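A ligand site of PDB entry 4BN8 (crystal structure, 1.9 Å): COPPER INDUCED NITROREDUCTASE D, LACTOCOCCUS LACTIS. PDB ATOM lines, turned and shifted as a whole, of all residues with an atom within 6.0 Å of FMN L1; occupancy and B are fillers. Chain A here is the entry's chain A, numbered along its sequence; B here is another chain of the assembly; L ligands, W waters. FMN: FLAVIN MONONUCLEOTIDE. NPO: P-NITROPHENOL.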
ATOM      1  N   ARG A   9     -32.523   9.058  -8.030  1.00  0.00           N
ATOM      2  CA  ARG A   9     -32.780   7.678  -8.415  1.00  0.00           C
ATOM      3  C   ARG A   9     -32.185   6.747  -7.391  1.00  0.00           C
ATOM      4  O   ARG A   9     -30.991   6.831  -7.077  1.00  0.00           O
ATOM      5  CB  ARG A   9     -32.154   7.372  -9.773  1.00  0.00           C
ATOM      6  CG  ARG A   9     -32.464   5.967 -10.277  1.00  0.00           C
ATOM      7  CD  ARG A   9     -31.245   5.318 -10.925  1.00  0.00           C
ATOM      8  NE  ARG A   9     -30.080   5.391 -10.052  1.00  0.00           N
ATOM      9  CZ  ARG A   9     -29.806   4.546  -9.058  1.00  0.00           C
ATOM     10  NH1 ARG A   9     -30.617   3.523  -8.796  1.00  0.00           N
ATOM     11  NH2 ARG A   9     -28.716   4.715  -8.329  1.00  0.00           N
ATOM     12  N   ARG A  10     -33.013   5.846  -6.860  1.00  0.00           N
ATOM     13  CA  ARG A  10     -32.571   4.847  -5.890  1.00  0.00           C
ATOM     14  C   ARG A  10     -33.334   3.544  -6.091  1.00  0.00           C
ATOM     15  O   ARG A  10     -34.404   3.509  -6.698  1.00  0.00           O
ATOM     16  CB  ARG A  10     -32.760   5.361  -4.461  1.00  0.00           C
ATOM     17  CG  ARG A  10     -31.926   6.597  -4.104  1.00  0.00           C
ATOM     18  CD  ARG A  10     -30.421   6.284  -4.050  1.00  0.00           C
ATOM     19  NE  ARG A  10     -30.147   5.159  -3.157  1.00  0.00           N
ATOM     20  CZ  ARG A  10     -30.122   5.244  -1.831  1.00  0.00           C
ATOM     21  NH1 ARG A  10     -30.336   6.399  -1.228  1.00  0.00           N
ATOM     22  NH2 ARG A  10     -29.875   4.156  -1.112  1.00  0.00           N
ATOM     23  N   THR A  11     -32.763   2.459  -5.574  1.00  0.00           N
ATOM     24  CA  THR A  11     -33.448   1.182  -5.536  1.00  0.00           C
ATOM     25  C   THR A  11     -34.548   1.260  -4.479  1.00  0.00           C
ATOM     26  O   THR A  11     -34.277   1.488  -3.296  1.00  0.00           O
ATOM     27  CB  THR A  11     -32.478   0.036  -5.193  1.00  0.00           C
ATOM     28  OG1 THR A  11     -31.623  -0.217  -6.315  1.00  0.00           O
ATOM     29  CG2 THR A  11     -33.234  -1.230  -4.821  1.00  0.00           C
ATOM     30  N   ILE A  12     -35.786   1.074  -4.911  1.00  0.00           N
ATOM     31  CA  ILE A  12     -36.940   1.059  -4.019  1.00  0.00           C
ATOM     32  C   ILE A  12     -37.612  -0.311  -4.117  1.00  0.00           C
ATOM     33  O   ILE A  12     -38.155  -0.658  -5.168  1.00  0.00           O
ATOM     34  CB  ILE A  12     -37.956   2.141  -4.414  1.00  0.00           C
ATOM     35  CG1 ILE A  12     -37.310   3.534  -4.364  1.00  0.00           C
ATOM     36  CG2 ILE A  12     -39.194   2.085  -3.521  1.00  0.00           C
ATOM     37  CD1 ILE A  12     -36.822   3.961  -2.999  1.00  0.00           C
ATOM     38  N   TYR A  13     -37.569  -1.083  -3.035  1.00  0.00           N
ATOM     39  CA  TYR A  13     -38.185  -2.411  -3.027  1.00  0.00           C
ATOM     40  C   TYR A  13     -39.672  -2.408  -2.673  1.00  0.00           C
ATOM     41  O   TYR A  13     -40.423  -3.247  -3.170  1.00  0.00           O
ATOM     42  CB  TYR A  13     -37.430  -3.372  -2.114  1.00  0.00           C
ATOM     43  CG  TYR A  13     -36.088  -3.774  -2.668  1.00  0.00           C
ATOM     44  CD1 TYR A  13     -35.993  -4.529  -3.837  1.00  0.00           C
ATOM     45  CD2 TYR A  13     -34.912  -3.383  -2.056  1.00  0.00           C
ATOM     46  CE1 TYR A  13     -34.765  -4.889  -4.362  1.00  0.00           C
ATOM     47  CE2 TYR A  13     -33.675  -3.733  -2.560  1.00  0.00           C
ATOM     48  CZ  TYR A  13     -33.608  -4.494  -3.720  1.00  0.00           C
ATOM     49  OH  TYR A  13     -32.367  -4.840  -4.233  1.00  0.00           O
ATOM     50  N   PHE A  91     -42.664  -7.861  -5.733  1.00  0.00           N
ATOM     51  CA  PHE A  91     -42.505  -7.445  -7.115  1.00  0.00           C
ATOM     52  C   PHE A  91     -43.867  -7.322  -7.799  1.00  0.00           C
ATOM     53  O   PHE A  91     -44.152  -6.342  -8.480  1.00  0.00           O
ATOM     54  CB  PHE A  91     -41.625  -8.434  -7.890  1.00  0.00           C
ATOM     55  CG  PHE A  91     -40.217  -8.501  -7.373  1.00  0.00           C
ATOM     56  CD1 PHE A  91     -39.508  -7.342  -7.110  1.00  0.00           C
ATOM     57  CD2 PHE A  91     -39.609  -9.719  -7.133  1.00  0.00           C
ATOM     58  CE1 PHE A  91     -38.211  -7.398  -6.615  1.00  0.00           C
ATOM     59  CE2 PHE A  91     -38.317  -9.786  -6.645  1.00  0.00           C
ATOM     60  CZ  PHE A  91     -37.616  -8.630  -6.387  1.00  0.00           C
ATOM     61  N   GLY A 130     -27.335  -1.390 -20.134  1.00  0.00           N
ATOM     62  CA  GLY A 130     -27.154  -0.662 -18.890  1.00  0.00           C
ATOM     63  C   GLY A 130     -27.615   0.771 -19.043  1.00  0.00           C
ATOM     64  O   GLY A 130     -28.348   1.310 -18.207  1.00  0.00           O
ATOM     65  N   VAL A 134     -30.803   2.470 -16.856  1.00  0.00           N
ATOM     66  CA  VAL A 134     -30.674   3.493 -15.816  1.00  0.00           C
ATOM     67  C   VAL A 134     -31.264   4.835 -16.228  1.00  0.00           C
ATOM     68  O   VAL A 134     -31.682   5.621 -15.381  1.00  0.00           O
ATOM     69  CB  VAL A 134     -29.219   3.723 -15.385  1.00  0.00           C
ATOM     70  CG1 VAL A 134     -28.613   2.437 -14.867  1.00  0.00           C
ATOM     71  CG2 VAL A 134     -28.396   4.304 -16.532  1.00  0.00           C
ATOM     72  N   TRP A 137     -34.886   4.262 -15.435  1.00  0.00           N
ATOM     73  CA  TRP A 137     -34.941   4.226 -13.975  1.00  0.00           C
ATOM     74  C   TRP A 137     -34.943   5.653 -13.421  1.00  0.00           C
ATOM     75  O   TRP A 137     -35.763   5.997 -12.563  1.00  0.00           O
ATOM     76  CB  TRP A 137     -33.705   3.459 -13.483  1.00  0.00           C
ATOM     77  CG  TRP A 137     -33.731   2.950 -12.075  1.00  0.00           C
ATOM     78  CD1 TRP A 137     -34.579   3.318 -11.063  1.00  0.00           C
ATOM     79  CD2 TRP A 137     -32.854   1.975 -11.522  1.00  0.00           C
ATOM     80  NE1 TRP A 137     -34.273   2.628  -9.918  1.00  0.00           N
ATOM     81  CE2 TRP A 137     -33.209   1.796 -10.173  1.00  0.00           C
ATOM     82  CE3 TRP A 137     -31.784   1.229 -12.032  1.00  0.00           C
ATOM     83  CZ2 TRP A 137     -32.548   0.904  -9.340  1.00  0.00           C
ATOM     84  CZ3 TRP A 137     -31.127   0.359 -11.203  1.00  0.00           C
ATOM     85  CH2 TRP A 137     -31.512   0.193  -9.871  1.00  0.00           C
ATOM     86  N   ASN A 148     -36.847  -0.953  -9.001  1.00  0.00           N
ATOM     87  CA  ASN A 148     -35.691  -1.789  -8.723  1.00  0.00           C
ATOM     88  C   ASN A 148     -35.440  -2.692  -9.918  1.00  0.00           C
ATOM     89  O   ASN A 148     -36.345  -2.991 -10.689  1.00  0.00           O
ATOM     90  CB  ASN A 148     -35.873  -2.582  -7.416  1.00  0.00           C
ATOM     91  CG  ASN A 148     -37.055  -3.535  -7.454  1.00  0.00           C
ATOM     92  OD1 ASN A 148     -36.990  -4.594  -8.077  1.00  0.00           O
ATOM     93  ND2 ASN A 148     -38.127  -3.168  -6.771  1.00  0.00           N
ATOM     94  N   LEU A 149     -34.190  -3.113 -10.067  1.00  0.00           N
ATOM     95  CA  LEU A 149     -33.743  -3.842 -11.233  1.00  0.00           C
ATOM     96  C   LEU A 149     -33.411  -5.276 -10.886  1.00  0.00           C
ATOM     97  O   LEU A 149     -32.549  -5.542 -10.040  1.00  0.00           O
ATOM     98  CB  LEU A 149     -32.498  -3.160 -11.828  1.00  0.00           C
ATOM     99  CG  LEU A 149     -31.908  -3.799 -13.078  1.00  0.00           C
ATOM    100  CD1 LEU A 149     -32.900  -3.808 -14.213  1.00  0.00           C
ATOM    101  CD2 LEU A 149     -30.637  -3.068 -13.480  1.00  0.00           C
ATOM    102  N   GLN A 150     -34.096  -6.209 -11.544  1.00  0.00           N
ATOM    103  CA  GLN A 150     -33.954  -7.633 -11.266  1.00  0.00           C
ATOM    104  C   GLN A 150     -33.395  -8.377 -12.473  1.00  0.00           C
ATOM    105  O   GLN A 150     -33.423  -7.874 -13.585  1.00  0.00           O
ATOM    106  CB  GLN A 150     -35.310  -8.225 -10.893  1.00  0.00           C
ATOM    107  CG  GLN A 150     -35.912  -7.613  -9.650  1.00  0.00           C
ATOM    108  CD  GLN A 150     -34.955  -7.688  -8.476  1.00  0.00           C
ATOM    109  OE1 GLN A 150     -34.322  -8.718  -8.252  1.00  0.00           O
ATOM    110  NE2 GLN A 150     -34.845  -6.601  -7.737  1.00  0.00           N
ATOM    111  N   HIS A 151     -32.889  -9.575 -12.233  1.00  0.00           N
ATOM    112  CA  HIS A 151     -32.323 -10.392 -13.292  1.00  0.00           C
ATOM    113  C   HIS A 151     -32.750 -11.856 -13.170  1.00  0.00           C
ATOM    114  O   HIS A 151     -32.027 -12.681 -12.636  1.00  0.00           O
ATOM    115  CB  HIS A 151     -30.809 -10.264 -13.293  1.00  0.00           C
ATOM    116  CG  HIS A 151     -30.336  -8.888 -13.631  1.00  0.00           C
ATOM    117  ND1 HIS A 151     -30.214  -7.888 -12.688  1.00  0.00           N
ATOM    118  CD2 HIS A 151     -30.017  -8.316 -14.816  1.00  0.00           C
ATOM    119  CE1 HIS A 151     -29.802  -6.780 -13.269  1.00  0.00           C
ATOM    120  NE2 HIS A 151     -29.681  -7.010 -14.565  1.00  0.00           N
ATOM    121  N   ALA A 185     -35.659   4.405   0.289  1.00  0.00           N
ATOM    122  CA  ALA A 185     -34.446   3.650   0.007  1.00  0.00           C
ATOM    123  C   ALA A 185     -33.679   3.440   1.306  1.00  0.00           C
ATOM    124  O   ALA A 185     -33.823   4.214   2.246  1.00  0.00           O
ATOM    125  CB  ALA A 185     -33.596   4.388  -1.002  1.00  0.00           C
ATOM    126  N   LYS A 188     -26.764   3.695   1.826  1.00  0.00           N
ATOM    127  CA  LYS A 188     -25.797   3.292   0.814  1.00  0.00           C
ATOM    128  C   LYS A 188     -24.456   3.955   1.094  1.00  0.00           C
ATOM    129  O   LYS A 188     -24.411   5.115   1.503  1.00  0.00           O
ATOM    130  CB  LYS A 188     -26.284   3.676  -0.598  1.00  0.00           C
ATOM    131  CG  LYS A 188     -25.309   3.289  -1.694  1.00  0.00           C
ATOM    132  CD  LYS A 188     -25.867   3.555  -3.088  1.00  0.00           C
ATOM    133  CE  LYS A 188     -26.317   4.994  -3.282  1.00  0.00           C
ATOM    134  NZ  LYS A 188     -26.543   5.273  -4.736  1.00  0.00           N
ATOM    135  N   PHE B  35     -23.018   8.833  -8.179  1.00  0.00           N
ATOM    136  CA  PHE B  35     -24.445   8.588  -8.064  1.00  0.00           C
ATOM    137  C   PHE B  35     -24.993   7.638  -9.125  1.00  0.00           C
ATOM    138  O   PHE B  35     -26.212   7.528  -9.306  1.00  0.00           O
ATOM    139  CB  PHE B  35     -25.178   9.929  -8.096  1.00  0.00           C
ATOM    140  CG  PHE B  35     -24.830  10.825  -6.935  1.00  0.00           C
ATOM    141  CD1 PHE B  35     -24.897  10.351  -5.637  1.00  0.00           C
ATOM    142  CD2 PHE B  35     -24.437  12.139  -7.147  1.00  0.00           C
ATOM    143  CE1 PHE B  35     -24.576  11.158  -4.567  1.00  0.00           C
ATOM    144  CE2 PHE B  35     -24.116  12.947  -6.077  1.00  0.00           C
ATOM    145  CZ  PHE B  35     -24.184  12.465  -4.795  1.00  0.00           C
ATOM    146  N   SER B  36     -24.093   6.930  -9.812  1.00  0.00           N
ATOM    147  CA  SER B  36     -24.486   5.899 -10.771  1.00  0.00           C
ATOM    148  C   SER B  36     -24.604   4.556 -10.078  1.00  0.00           C
ATOM    149  O   SER B  36     -23.746   4.198  -9.279  1.00  0.00           O
ATOM    150  CB  SER B  36     -23.457   5.796 -11.897  1.00  0.00           C
ATOM    151  OG  SER B  36     -23.393   6.987 -12.665  1.00  0.00           O
ATOM    152  N   PRO B  37     -25.671   3.788 -10.382  1.00  0.00           N
ATOM    153  CA  PRO B  37     -25.833   2.477  -9.753  1.00  0.00           C
ATOM    154  C   PRO B  37     -24.947   1.402 -10.374  1.00  0.00           C
ATOM    155  O   PRO B  37     -24.662   1.439 -11.573  1.00  0.00           O
ATOM    156  CB  PRO B  37     -27.313   2.166 -10.018  1.00  0.00           C
ATOM    157  CG  PRO B  37     -27.592   2.845 -11.324  1.00  0.00           C
ATOM    158  CD  PRO B  37     -26.770   4.113 -11.305  1.00  0.00           C
ATOM    159  N   THR B  38     -24.526   0.446  -9.549  1.00  0.00           N
ATOM    160  CA  THR B  38     -23.754  -0.701  -9.981  1.00  0.00           C
ATOM    161  C   THR B  38     -24.232  -1.940  -9.242  1.00  0.00           C
ATOM    162  O   THR B  38     -24.667  -1.830  -8.086  1.00  0.00           O
ATOM    163  CB  THR B  38     -22.252  -0.519  -9.708  1.00  0.00           C
ATOM    164  OG1 THR B  38     -22.052  -0.222  -8.319  1.00  0.00           O
ATOM    165  CG2 THR B  38     -21.683   0.602 -10.560  1.00  0.00           C
ATOM    166  N   ALA B  39     -24.154  -3.105  -9.874  1.00  0.00           N
ATOM    167  CA  ALA B  39     -24.590  -4.332  -9.231  1.00  0.00           C
ATOM    168  C   ALA B  39     -23.927  -4.477  -7.851  1.00  0.00           C
ATOM    169  O   ALA B  39     -22.715  -4.289  -7.718  1.00  0.00           O
ATOM    170  CB  ALA B  39     -24.266  -5.533 -10.095  1.00  0.00           C
ATOM    171  N   PHE B  40     -24.734  -4.762  -6.840  1.00  0.00           N
ATOM    172  CA  PHE B  40     -24.218  -5.035  -5.492  1.00  0.00           C
ATOM    173  C   PHE B  40     -23.511  -3.812  -4.935  1.00  0.00           C
ATOM    174  O   PHE B  40     -22.748  -3.922  -3.961  1.00  0.00           O
ATOM    175  CB  PHE B  40     -23.236  -6.208  -5.519  1.00  0.00           C
ATOM    176  CG  PHE B  40     -23.883  -7.570  -5.481  1.00  0.00           C
ATOM    177  CD1 PHE B  40     -24.512  -8.085  -6.605  1.00  0.00           C
ATOM    178  CD2 PHE B  40     -23.817  -8.350  -4.333  1.00  0.00           C
ATOM    179  CE1 PHE B  40     -25.092  -9.345  -6.571  1.00  0.00           C
ATOM    180  CE2 PHE B  40     -24.396  -9.611  -4.299  1.00  0.00           C
ATOM    181  CZ  PHE B  40     -25.034 -10.108  -5.418  1.00  0.00           C
ATOM    182  N   ASN B  41     -23.759  -2.645  -5.531  1.00  0.00           N
ATOM    183  CA  ASN B  41     -23.066  -1.425  -5.149  1.00  0.00           C
ATOM    184  C   ASN B  41     -21.562  -1.647  -5.219  1.00  0.00           C
ATOM    185  O   ASN B  41     -20.813  -1.127  -4.399  1.00  0.00           O
ATOM    186  CB  ASN B  41     -23.472  -0.996  -3.740  1.00  0.00           C
ATOM    187  CG  ASN B  41     -23.066   0.427  -3.424  1.00  0.00           C
ATOM    188  OD1 ASN B  41     -23.017   1.288  -4.301  1.00  0.00           O
ATOM    189  ND2 ASN B  41     -22.751   0.684  -2.147  1.00  0.00           N
ATOM    190  N   SER B  42     -21.150  -2.432  -6.199  1.00  0.00           N
ATOM    191  CA  SER B  42     -19.748  -2.853  -6.340  1.00  0.00           C
ATOM    192  C   SER B  42     -18.814  -1.716  -6.804  1.00  0.00           C
ATOM    193  O   SER B  42     -17.608  -1.766  -6.562  1.00  0.00           O
ATOM    194  CB  SER B  42     -19.648  -4.041  -7.299  1.00  0.00           C
ATOM    195  OG  SER B  42     -20.243  -3.762  -8.558  1.00  0.00           O
ATOM    196  N   TRP B 124     -22.576  -7.401 -15.730  1.00  0.00           N
ATOM    197  CA  TRP B 124     -23.031  -6.225 -14.997  1.00  0.00           C
ATOM    198  C   TRP B 124     -21.955  -5.157 -14.938  1.00  0.00           C
ATOM    199  O   TRP B 124     -22.255  -3.965 -14.896  1.00  0.00           O
ATOM    200  CB  TRP B 124     -23.475  -6.622 -13.590  1.00  0.00           C
ATOM    201  CG  TRP B 124     -24.698  -7.480 -13.587  1.00  0.00           C
ATOM    202  CD1 TRP B 124     -25.666  -7.530 -14.540  1.00  0.00           C
ATOM    203  CD2 TRP B 124     -25.076  -8.430 -12.578  1.00  0.00           C
ATOM    204  NE1 TRP B 124     -26.631  -8.455 -14.190  1.00  0.00           N
ATOM    205  CE2 TRP B 124     -26.292  -9.009 -12.988  1.00  0.00           C
ATOM    206  CE3 TRP B 124     -24.510  -8.834 -11.368  1.00  0.00           C
ATOM    207  CZ2 TRP B 124     -26.944  -9.982 -12.233  1.00  0.00           C
ATOM    208  CZ3 TRP B 124     -25.154  -9.791 -10.614  1.00  0.00           C
ATOM    209  CH2 TRP B 124     -26.367 -10.361 -11.055  1.00  0.00           C
ATOM    210  N   SER B 125     -20.696  -5.588 -14.956  1.00  0.00           N
ATOM    211  CA  SER B 125     -19.582  -4.649 -14.979  1.00  0.00           C
ATOM    212  C   SER B 125     -19.559  -3.872 -16.293  1.00  0.00           C
ATOM    213  O   SER B 125     -19.387  -2.660 -16.306  1.00  0.00           O
ATOM    214  CB  SER B 125     -18.259  -5.381 -14.791  1.00  0.00           C
ATOM    215  OG  SER B 125     -17.156  -4.510 -14.961  1.00  0.00           O
ATOM    216  N   GLN B 127     -22.120  -3.396 -18.328  1.00  0.00           N
ATOM    217  CA  GLN B 127     -23.271  -2.507 -18.218  1.00  0.00           C
ATOM    218  C   GLN B 127     -22.923  -1.279 -17.386  1.00  0.00           C
ATOM    219  O   GLN B 127     -23.232  -0.145 -17.762  1.00  0.00           O
ATOM    220  CB  GLN B 127     -24.480  -3.268 -17.645  1.00  0.00           C
ATOM    221  CG  GLN B 127     -25.036  -4.313 -18.624  1.00  0.00           C
ATOM    222  CD  GLN B 127     -26.124  -5.201 -18.048  1.00  0.00           C
ATOM    223  OE1 GLN B 127     -26.510  -5.057 -16.889  1.00  0.00           O
ATOM    224  NE2 GLN B 127     -26.611  -6.123 -18.863  1.00  0.00           N
ATOM    225  N   GLY B 128     -22.235  -1.510 -16.266  1.00  0.00           N
ATOM    226  CA  GLY B 128     -21.810  -0.429 -15.388  1.00  0.00           C
ATOM    227  C   GLY B 128     -20.898   0.596 -16.060  1.00  0.00           C
ATOM    228  O   GLY B 128     -20.960   1.784 -15.769  1.00  0.00           O
ATOM    229  N   ILE B 131     -23.075   2.769 -18.183  1.00  0.00           N
ATOM    230  CA  ILE B 131     -23.830   3.617 -17.266  1.00  0.00           C
ATOM    231  C   ILE B 131     -23.046   4.844 -16.840  1.00  0.00           C
ATOM    232  O   ILE B 131     -23.503   5.976 -17.007  1.00  0.00           O
ATOM    233  CB  ILE B 131     -24.267   2.815 -16.030  1.00  0.00           C
ATOM    234  CG1 ILE B 131     -25.334   1.789 -16.425  1.00  0.00           C
ATOM    235  CG2 ILE B 131     -24.805   3.743 -14.952  1.00  0.00           C
ATOM    236  CD1 ILE B 131     -25.668   0.782 -15.339  1.00  0.00           C
HETATM  237  N1  FMN L   1     -30.591  -5.072  -7.512  1.00  0.00           N
HETATM  238  C2  FMN L   1     -31.383  -6.319  -7.231  1.00  0.00           C
HETATM  239  O2  FMN L   1     -32.160  -6.352  -6.335  1.00  0.00           O
HETATM  240  N3  FMN L   1     -31.193  -7.480  -8.052  1.00  0.00           N
HETATM  241  C4  FMN L   1     -30.306  -7.480  -9.094  1.00  0.00           C
HETATM  242  O4  FMN L   1     -30.195  -8.430  -9.787  1.00  0.00           O
HETATM  243  C4A FMN L   1     -29.530  -6.263  -9.373  1.00  0.00           C
HETATM  244  N5  FMN L   1     -28.702  -6.234 -10.332  1.00  0.00           N
HETATM  245  C5A FMN L   1     -28.146  -4.901 -10.785  1.00  0.00           C
HETATM  246  C6  FMN L   1     -27.405  -4.809 -12.113  1.00  0.00           C
HETATM  247  C7  FMN L   1     -26.935  -3.644 -12.519  1.00  0.00           C
HETATM  248  C7M FMN L   1     -26.186  -3.549 -13.841  1.00  0.00           C
HETATM  249  C8  FMN L   1     -27.134  -2.391 -11.669  1.00  0.00           C
HETATM  250  C8M FMN L   1     -26.604  -1.047 -12.165  1.00  0.00           C
HETATM  251  C9  FMN L   1     -27.775  -2.467 -10.517  1.00  0.00           C
HETATM  252  C9A FMN L   1     -28.322  -3.803 -10.037  1.00  0.00           C
HETATM  253  N10 FMN L   1     -29.012  -3.886  -8.779  1.00  0.00           N
HETATM  254  C10 FMN L   1     -29.727  -5.050  -8.506  1.00  0.00           C
HETATM  255  C1' FMN L   1     -29.214  -2.711  -7.945  1.00  0.00           C
HETATM  256  C2' FMN L   1     -27.917  -2.287  -7.249  1.00  0.00           C
HETATM  257  O2' FMN L   1     -27.615  -3.162  -6.185  1.00  0.00           O
HETATM  258  C3' FMN L   1     -28.107  -0.880  -6.693  1.00  0.00           C
HETATM  259  O3' FMN L   1     -28.323   0.002  -7.762  1.00  0.00           O
HETATM  260  C4' FMN L   1     -26.855  -0.467  -5.915  1.00  0.00           C
HETATM  261  O4' FMN L   1     -26.792  -1.184  -4.713  1.00  0.00           O
HETATM  262  C5' FMN L   1     -26.903   1.023  -5.578  1.00  0.00           C
HETATM  263  O5' FMN L   1     -28.078   1.275  -4.865  1.00  0.00           O
HETATM  264  P   FMN L   1     -29.152   2.333  -5.514  1.00  0.00           P
HETATM  265  O1P FMN L   1     -28.473   3.582  -5.869  1.00  0.00           O
HETATM  266  O2P FMN L   1     -29.791   1.673  -6.870  1.00  0.00           O
HETATM  267  O3P FMN L   1     -30.309   2.639  -4.395  1.00  0.00           O
HETATM  268  C1  NPO L   2     -29.100  -9.807  -6.174  1.00  0.00           C
HETATM  269  C2  NPO L   2     -28.313  -9.643  -7.313  1.00  0.00           C
HETATM  270  C3  NPO L   2     -27.674  -8.437  -7.539  1.00  0.00           C
HETATM  271  C4  NPO L   2     -27.835  -7.402  -6.623  1.00  0.00           C
HETATM  272  C5  NPO L   2     -28.606  -7.568  -5.490  1.00  0.00           C
HETATM  273  C6  NPO L   2     -29.249  -8.765  -5.261  1.00  0.00           C
HETATM  274  OH  NPO L   2     -27.195  -6.203  -6.828  1.00  0.00           O
HETATM  275  N1  NPO L   2     -29.755 -11.056  -5.940  1.00  0.00           N
HETATM  276  O2  NPO L   2     -29.824 -11.886  -6.835  1.00  0.00           O
HETATM  277  O3  NPO L   2     -30.262 -11.291  -4.770  1.00  0.00           O
HETATM  278  O   HOH W   1     -29.884  -3.628  -4.408  1.00  0.00           O
HETATM  279  O   HOH W   2     -32.452  -2.493  -7.709  1.00  0.00           O
HETATM  280  O   HOH W   3     -27.929  -0.353  -2.221  1.00  0.00           O
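The guanidinium group of Arg 9 is in salt-bridge range of an oxygen (O1P) of FMN L1 (2.7 Å). An oxygen (O4') of FMN L1 lies within hydrogen-bond range of the backbone NH of Asn 41 of chain B, at 3.5 Å. N of Thr 11 sits at hydrogen-bond distance from O3P of FMN L1 (2.7 Å). An oxygen (O2') of FMN L1 lies within hydrogen-bond range of the backbone NH (N) of Phe 40 of chain B, at 3.4 Å. A ring nitrogen (ND1) of His 151 lies within hydrogen-bond range of an oxygen (O4) of FMN L1 (3.0 Å). O of Leu 149 is in hydrogen-bond range of N3 of FMN L1 (3.1 Å). The side-chain amino group (NZ) of Lys 188 lies within salt-bridge range of an oxygen (O1P) of FMN L1 (2.8 Å). OH of NPO L2 lies within hydrogen-bond range of N of Phe 40 of chain B (2.9 Å). The side-chain hydroxyl (OH) of Tyr 13 sits at hydrogen-bond distance from an oxygen (O2) of FMN L1 (2.6 Å). The side-chain amide nitrogen (NE2) of Gln 150 sits at hydrogen-bond distance from an oxygen (O2) of FMN L1 (3.0 Å). NE of Arg 10 lies within salt-bridge range of O3P of FMN L1, 2.8 Å away. OG1 of Thr 11 lies within hydrogen-bond range of O2P of FMN L1 (2.7 Å).
An oxygen (O2') of FMN L1 sits at hydrogen-bond distance from an oxygen (OH) of NPO L2 (3.1 Å).
OG of Ser 42 of chain B lies within hydrogen-bond range of O of Ala 39 of chain B (2.7 Å). The backbone NH (N) of Ser 42 of chain B is in hydrogen-bond range of the side-chain hydroxyl (OG1) of Thr 38 of chain B (3.2 Å). NE1 of Trp 137 sits at hydrogen-bond distance from O of Arg 10. The indole nitrogen (NE1) of Trp 124 of chain B lies within hydrogen-bond range of a ring nitrogen (NE2) of His 151 (3.4 Å). The side-chain amide nitrogen (NE2) of Gln 150 is in hydrogen-bond range of the side-chain amide oxygen (OD1) of Asn 148 (3.0 Å).
Trp 137 touches FMN L1 (CH2 to O2P, 3.8 Å). Pro 37 of chain B touches FMN L1. Thr 38 of chain B touches FMN L1 (O to C4', 3.4 Å). N of Ala 39 of chain B touches C8 of FMN L1, at 3.6 Å. Gln 127 of chain B touches FMN L1. Ile 131 of chain B touches FMN L1. Within 4 Å of FMN L1: Arg 9, Arg 10, Thr 11, Tyr 13, Trp 137, Leu 149, Gln 150, His 151, Lys 188, Pro 37 of chain B, Thr 38 of chain B, Ala 39 of chain B, Phe 40 of chain B, Asn 41 of chain B, Gln 127 of chain B and Ile 131 of chain B. The nearest printed residue that does not touch FMN L1 is Trp 124 of chain B (4.04 Å).
Water W1 lies within hydrogen-bond range of OH of Tyr 13 (2.8 Å) and O2' of FMN L1 (2.9 Å). Water W2 lies within hydrogen-bond range of OG1 of Thr 11 (2.8 Å), N of Leu 149 (3.0 Å) and N1 of FMN L1 (3.2 Å).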
